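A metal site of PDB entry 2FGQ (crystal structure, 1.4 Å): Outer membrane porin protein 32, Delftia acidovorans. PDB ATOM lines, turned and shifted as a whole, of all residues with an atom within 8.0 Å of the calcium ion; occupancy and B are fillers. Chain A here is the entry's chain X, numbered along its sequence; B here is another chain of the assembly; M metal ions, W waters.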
ATOM      1  N   ASN A  13      -8.451 -26.171 -12.468  1.00  0.00           N
ATOM      2  CA  ASN A  13      -9.139 -26.622 -13.678  1.00  0.00           C
ATOM      3  C   ASN A  13     -10.403 -25.820 -13.944  1.00  0.00           C
ATOM      4  O   ASN A  13     -10.906 -25.086 -13.108  1.00  0.00           O
ATOM      5  CB  ASN A  13      -9.476 -28.150 -13.620  1.00  0.00           C
ATOM      6  CG  ASN A  13     -10.244 -28.538 -12.361  1.00  0.00           C
ATOM      7  OD1 ASN A  13     -11.343 -28.001 -12.094  1.00  0.00           O
ATOM      8  ND2 ASN A  13      -9.713 -29.495 -11.579  1.00  0.00           N
ATOM      9  N   TYR A  27     -20.971 -25.389 -13.917  1.00  0.00           N
ATOM     10  CA  TYR A  27     -19.619 -25.316 -14.393  1.00  0.00           C
ATOM     11  C   TYR A  27     -18.876 -24.224 -13.672  1.00  0.00           C
ATOM     12  O   TYR A  27     -19.463 -23.341 -13.051  1.00  0.00           O
ATOM     13  CB  TYR A  27     -19.612 -25.143 -15.882  1.00  0.00           C
ATOM     14  CG  TYR A  27     -20.278 -23.883 -16.300  1.00  0.00           C
ATOM     15  CD1 TYR A  27     -19.557 -22.736 -16.440  1.00  0.00           C
ATOM     16  CD2 TYR A  27     -21.656 -23.842 -16.523  1.00  0.00           C
ATOM     17  CE1 TYR A  27     -20.159 -21.551 -16.822  1.00  0.00           C
ATOM     18  CE2 TYR A  27     -22.285 -22.622 -16.866  1.00  0.00           C
ATOM     19  CZ  TYR A  27     -21.512 -21.491 -17.006  1.00  0.00           C
ATOM     20  OH  TYR A  27     -22.076 -20.263 -17.376  1.00  0.00           O
ATOM     21  N   GLY A  28     -17.564 -24.311 -13.718  1.00  0.00           N
ATOM     22  CA  GLY A  28     -16.795 -23.427 -12.850  1.00  0.00           C
ATOM     23  C   GLY A  28     -15.317 -23.647 -12.895  1.00  0.00           C
ATOM     24  O   GLY A  28     -14.803 -24.400 -13.727  1.00  0.00           O
ATOM     25  N   LEU A  29     -14.636 -22.985 -11.958  1.00  0.00           N
ATOM     26  CA  LEU A  29     -13.201 -23.134 -11.775  1.00  0.00           C
ATOM     27  C   LEU A  29     -13.063 -24.039 -10.554  1.00  0.00           C
ATOM     28  O   LEU A  29     -13.536 -23.672  -9.485  1.00  0.00           O
ATOM     29  CB  LEU A  29     -12.497 -21.796 -11.566  1.00  0.00           C
ATOM     30  CG  LEU A  29     -10.966 -21.889 -11.739  1.00  0.00           C
ATOM     31  CD1 LEU A  29     -10.623 -21.923 -13.222  1.00  0.00           C
ATOM     32  CD2 LEU A  29     -10.261 -20.787 -11.009  1.00  0.00           C
ATOM     33  N   GLY A  30     -12.438 -25.172 -10.696  1.00  0.00           N
ATOM     34  CA  GLY A  30     -12.212 -26.104  -9.613  1.00  0.00           C
ATOM     35  C   GLY A  30     -10.747 -26.432  -9.450  1.00  0.00           C
ATOM     36  O   GLY A  30      -9.864 -25.782  -9.977  1.00  0.00           O
ATOM     37  N   THR A  31     -10.486 -27.455  -8.641  1.00  0.00           N
ATOM     38  CA  THR A  31      -9.122 -27.812  -8.285  1.00  0.00           C
ATOM     39  C   THR A  31      -8.871 -29.292  -8.285  1.00  0.00           C
ATOM     40  O   THR A  31      -9.820 -30.104  -8.218  1.00  0.00           O
ATOM     41  CB  THR A  31      -8.745 -27.242  -6.886  1.00  0.00           C
ATOM     42  OG1 THR A  31      -9.581 -27.834  -5.854  1.00  0.00           O
ATOM     43  CG2 THR A  31      -8.908 -25.714  -6.825  1.00  0.00           C
ATOM     44  N   GLY A  63      -6.974 -23.330  -4.993  1.00  0.00           N
ATOM     45  CA  GLY A  63      -6.583 -22.171  -5.774  1.00  0.00           C
ATOM     46  C   GLY A  63      -7.757 -21.366  -6.263  1.00  0.00           C
ATOM     47  O   GLY A  63      -7.612 -20.178  -6.497  1.00  0.00           O
ATOM     48  N   ASP A  64      -8.932 -21.952  -6.370  1.00  0.00           N
ATOM     49  CA  ASP A  64     -10.091 -21.192  -6.843  1.00  0.00           C
ATOM     50  C   ASP A  64     -10.630 -20.171  -5.837  1.00  0.00           C
ATOM     51  O   ASP A  64     -11.241 -19.190  -6.260  1.00  0.00           O
ATOM     52  CB  ASP A  64     -11.218 -22.117  -7.345  1.00  0.00           C
ATOM     53  CG  ASP A  64     -11.738 -23.086  -6.289  1.00  0.00           C
ATOM     54  OD1 ASP A  64     -11.044 -23.435  -5.286  1.00  0.00           O
ATOM     55  OD2 ASP A  64     -12.926 -23.497  -6.417  1.00  0.00           O
ATOM     56  N   ASP A  65     -10.372 -20.366  -4.555  1.00  0.00           N
ATOM     57  CA  ASP A  65     -10.820 -19.444  -3.525  1.00  0.00           C
ATOM     58  C   ASP A  65      -9.782 -19.006  -2.523  1.00  0.00           C
ATOM     59  O   ASP A  65     -10.121 -18.387  -1.519  1.00  0.00           O
ATOM     60  CB  ASP A  65     -12.119 -19.905  -2.872  1.00  0.00           C
ATOM     61  CG  ASP A  65     -11.934 -21.024  -1.883  1.00  0.00           C
ATOM     62  OD1 ASP A  65     -10.793 -21.395  -1.495  1.00  0.00           O
ATOM     63  OD2 ASP A  65     -12.938 -21.557  -1.378  1.00  0.00           O
ATOM     64  N   ALA A 307     -16.337 -33.122  -8.750  1.00  0.00           N
ATOM     65  CA  ALA A 307     -15.672 -31.992  -9.422  1.00  0.00           C
ATOM     66  C   ALA A 307     -15.353 -30.952  -8.341  1.00  0.00           C
ATOM     67  O   ALA A 307     -16.156 -30.033  -8.111  1.00  0.00           O
ATOM     68  CB  ALA A 307     -16.543 -31.368 -10.525  1.00  0.00           C
ATOM     69  N   LYS A 308     -14.239 -31.135  -7.634  1.00  0.00           N
ATOM     70  CA  LYS A 308     -13.904 -30.327  -6.460  1.00  0.00           C
ATOM     71  C   LYS A 308     -13.835 -28.862  -6.867  1.00  0.00           C
ATOM     72  O   LYS A 308     -13.171 -28.523  -7.853  1.00  0.00           O
ATOM     73  CB  LYS A 308     -12.585 -30.753  -5.868  1.00  0.00           C
ATOM     74  CG  LYS A 308     -12.209 -30.012  -4.607  1.00  0.00           C
ATOM     75  CD  LYS A 308     -10.930 -30.608  -3.965  1.00  0.00           C
ATOM     76  CE  LYS A 308     -11.231 -31.763  -3.021  1.00  0.00           C
ATOM     77  NZ  LYS A 308     -10.007 -32.393  -2.470  1.00  0.00           N
ATOM     78  N   GLY A 309     -14.504 -28.029  -6.086  1.00  0.00           N
ATOM     79  CA  GLY A 309     -14.563 -26.591  -6.315  1.00  0.00           C
ATOM     80  C   GLY A 309     -15.630 -26.190  -7.295  1.00  0.00           C
ATOM     81  O   GLY A 309     -15.780 -24.993  -7.550  1.00  0.00           O
ATOM     82  N   VAL A 310     -16.352 -27.154  -7.851  1.00  0.00           N
ATOM     83  CA  VAL A 310     -17.444 -26.830  -8.773  1.00  0.00           C
ATOM     84  C   VAL A 310     -18.746 -27.452  -8.289  1.00  0.00           C
ATOM     85  O   VAL A 310     -19.679 -26.747  -7.931  1.00  0.00           O
ATOM     86  CB  VAL A 310     -17.119 -27.182 -10.250  1.00  0.00           C
ATOM     87  CG1 VAL A 310     -18.324 -26.890 -11.161  1.00  0.00           C
ATOM     88  CG2 VAL A 310     -15.926 -26.373 -10.700  1.00  0.00           C
ATOM     89  N   TYR A 311     -18.792 -28.785  -8.269  1.00  0.00           N
ATOM     90  CA  TYR A 311     -19.943 -29.479  -7.714  1.00  0.00           C
ATOM     91  C   TYR A 311     -19.495 -30.902  -7.382  1.00  0.00           C
ATOM     92  O   TYR A 311     -18.970 -31.613  -8.249  1.00  0.00           O
ATOM     93  CB  TYR A 311     -21.119 -29.508  -8.694  1.00  0.00           C
ATOM     94  CG  TYR A 311     -22.352 -30.129  -8.049  1.00  0.00           C
ATOM     95  CD1 TYR A 311     -23.042 -29.477  -7.044  1.00  0.00           C
ATOM     96  CD2 TYR A 311     -22.746 -31.445  -8.373  1.00  0.00           C
ATOM     97  CE1 TYR A 311     -24.114 -30.078  -6.399  1.00  0.00           C
ATOM     98  CE2 TYR A 311     -23.849 -32.059  -7.723  1.00  0.00           C
ATOM     99  CZ  TYR A 311     -24.515 -31.371  -6.744  1.00  0.00           C
ATOM    100  OH  TYR A 311     -25.592 -31.923  -6.086  1.00  0.00           O
ATOM    101  N   ASN B 135     -13.134 -14.918  -6.628  1.00  0.00           N
ATOM    102  CA  ASN B 135     -12.978 -16.382  -6.716  1.00  0.00           C
ATOM    103  C   ASN B 135     -13.230 -16.854  -8.128  1.00  0.00           C
ATOM    104  O   ASN B 135     -13.933 -16.207  -8.918  1.00  0.00           O
ATOM    105  CB  ASN B 135     -13.995 -17.075  -5.790  1.00  0.00           C
ATOM    106  CG  ASN B 135     -13.834 -16.731  -4.295  1.00  0.00           C
ATOM    107  OD1 ASN B 135     -14.813 -16.700  -3.505  1.00  0.00           O
ATOM    108  ND2 ASN B 135     -12.663 -16.516  -3.904  1.00  0.00           N
ATOM    109  N   ASN B 136     -12.665 -18.011  -8.435  1.00  0.00           N
ATOM    110  CA  ASN B 136     -13.031 -18.739  -9.670  1.00  0.00           C
ATOM    111  C   ASN B 136     -12.720 -17.938 -10.906  1.00  0.00           C
ATOM    112  O   ASN B 136     -13.414 -18.046 -11.927  1.00  0.00           O
ATOM    113  CB  ASN B 136     -14.521 -19.055  -9.670  1.00  0.00           C
ATOM    114  CG  ASN B 136     -14.959 -19.750  -8.354  1.00  0.00           C
ATOM    115  OD1 ASN B 136     -14.277 -20.660  -7.864  1.00  0.00           O
ATOM    116  ND2 ASN B 136     -16.059 -19.282  -7.762  1.00  0.00           N
ATOM    117  N   LEU B 137     -11.604 -17.209 -10.857  1.00  0.00           N
ATOM    118  CA  LEU B 137     -11.202 -16.253 -11.885  1.00  0.00           C
ATOM    119  C   LEU B 137     -10.206 -16.841 -12.930  1.00  0.00           C
ATOM    120  O   LEU B 137      -9.254 -17.551 -12.590  1.00  0.00           O
ATOM    121  CB  LEU B 137     -10.575 -15.049 -11.174  1.00  0.00           C
ATOM    122  CG  LEU B 137     -10.059 -13.927 -12.078  1.00  0.00           C
ATOM    123  CD1 LEU B 137     -11.191 -13.193 -12.795  1.00  0.00           C
ATOM    124  CD2 LEU B 137      -9.273 -12.972 -11.227  1.00  0.00           C
ATOM    125  N   PHE B 156     -16.334 -17.360 -12.727  1.00  0.00           N
ATOM    126  CA  PHE B 156     -17.520 -18.174 -12.698  1.00  0.00           C
ATOM    127  C   PHE B 156     -18.330 -18.002 -11.397  1.00  0.00           C
ATOM    128  O   PHE B 156     -17.795 -18.015 -10.306  1.00  0.00           O
ATOM    129  CB  PHE B 156     -17.138 -19.652 -12.807  1.00  0.00           C
ATOM    130  CG  PHE B 156     -16.419 -20.019 -14.075  1.00  0.00           C
ATOM    131  CD1 PHE B 156     -15.047 -19.987 -14.142  1.00  0.00           C
ATOM    132  CD2 PHE B 156     -17.123 -20.450 -15.184  1.00  0.00           C
ATOM    133  CE1 PHE B 156     -14.396 -20.350 -15.304  1.00  0.00           C
ATOM    134  CE2 PHE B 156     -16.469 -20.812 -16.371  1.00  0.00           C
ATOM    135  CZ  PHE B 156     -15.107 -20.748 -16.437  1.00  0.00           C
ATOM    136  N   ASP B 157     -19.633 -17.905 -11.535  1.00  0.00           N
ATOM    137  CA  ASP B 157     -20.541 -17.861 -10.405  1.00  0.00           C
ATOM    138  C   ASP B 157     -20.801 -19.200  -9.774  1.00  0.00           C
ATOM    139  O   ASP B 157     -21.045 -19.259  -8.565  1.00  0.00           O
ATOM    140  CB  ASP B 157     -21.873 -17.239 -10.816  1.00  0.00           C
ATOM    141  CG  ASP B 157     -22.451 -17.874 -12.028  1.00  0.00           C
ATOM    142  OD1 ASP B 157     -23.296 -18.812 -11.928  1.00  0.00           O
ATOM    143  OD2 ASP B 157     -22.065 -17.514 -13.164  1.00  0.00           O
ATOM    144  N   GLU B 158     -20.743 -20.238 -10.578  1.00  0.00           N
ATOM    145  CA  GLU B 158     -20.960 -21.611 -10.089  1.00  0.00           C
ATOM    146  C   GLU B 158     -22.335 -21.796  -9.433  1.00  0.00           C
ATOM    147  O   GLU B 158     -22.523 -22.592  -8.504  1.00  0.00           O
ATOM    148  CB  GLU B 158     -19.827 -22.044  -9.130  1.00  0.00           C
ATOM    149  CG  GLU B 158     -18.502 -21.896  -9.831  1.00  0.00           C
ATOM    150  CD  GLU B 158     -17.262 -22.208  -9.028  1.00  0.00           C
ATOM    151  OE1 GLU B 158     -17.336 -22.352  -7.784  1.00  0.00           O
ATOM    152  OE2 GLU B 158     -16.183 -22.247  -9.687  1.00  0.00           O
HETATM  153 CA    CA M   1     -14.877 -22.910  -7.678  1.00  0.00          CA
HETATM  154  O   HOH W   1     -15.538 -22.432  -5.349  1.00  0.00           O
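The backbone carbonyl oxygen (O) of Asn 136 of chain B lies within hydrogen-bond range of the backbone NH (N) of Phe 156 of chain B, at 3.1 Å.
The calcium ion is bound by O of Gly 309 (2.3 Å), OD1 of Asn 136 of chain B (2.3 Å), O of Leu 29 (2.4 Å), OD2 of Asp 64 (2.4 Å), water W1 (2.5 Å), OE2 of Glu 158 of chain B (2.5 Å) and OE1 of Glu 158 of chain B (2.5 Å). The calcium ion has seven donor atoms within binding distance.
Within 4 Å of the calcium ion: Leu 29, Asp 64, Gly 309, Asn 136 of chain B and Glu 158 of chain B.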
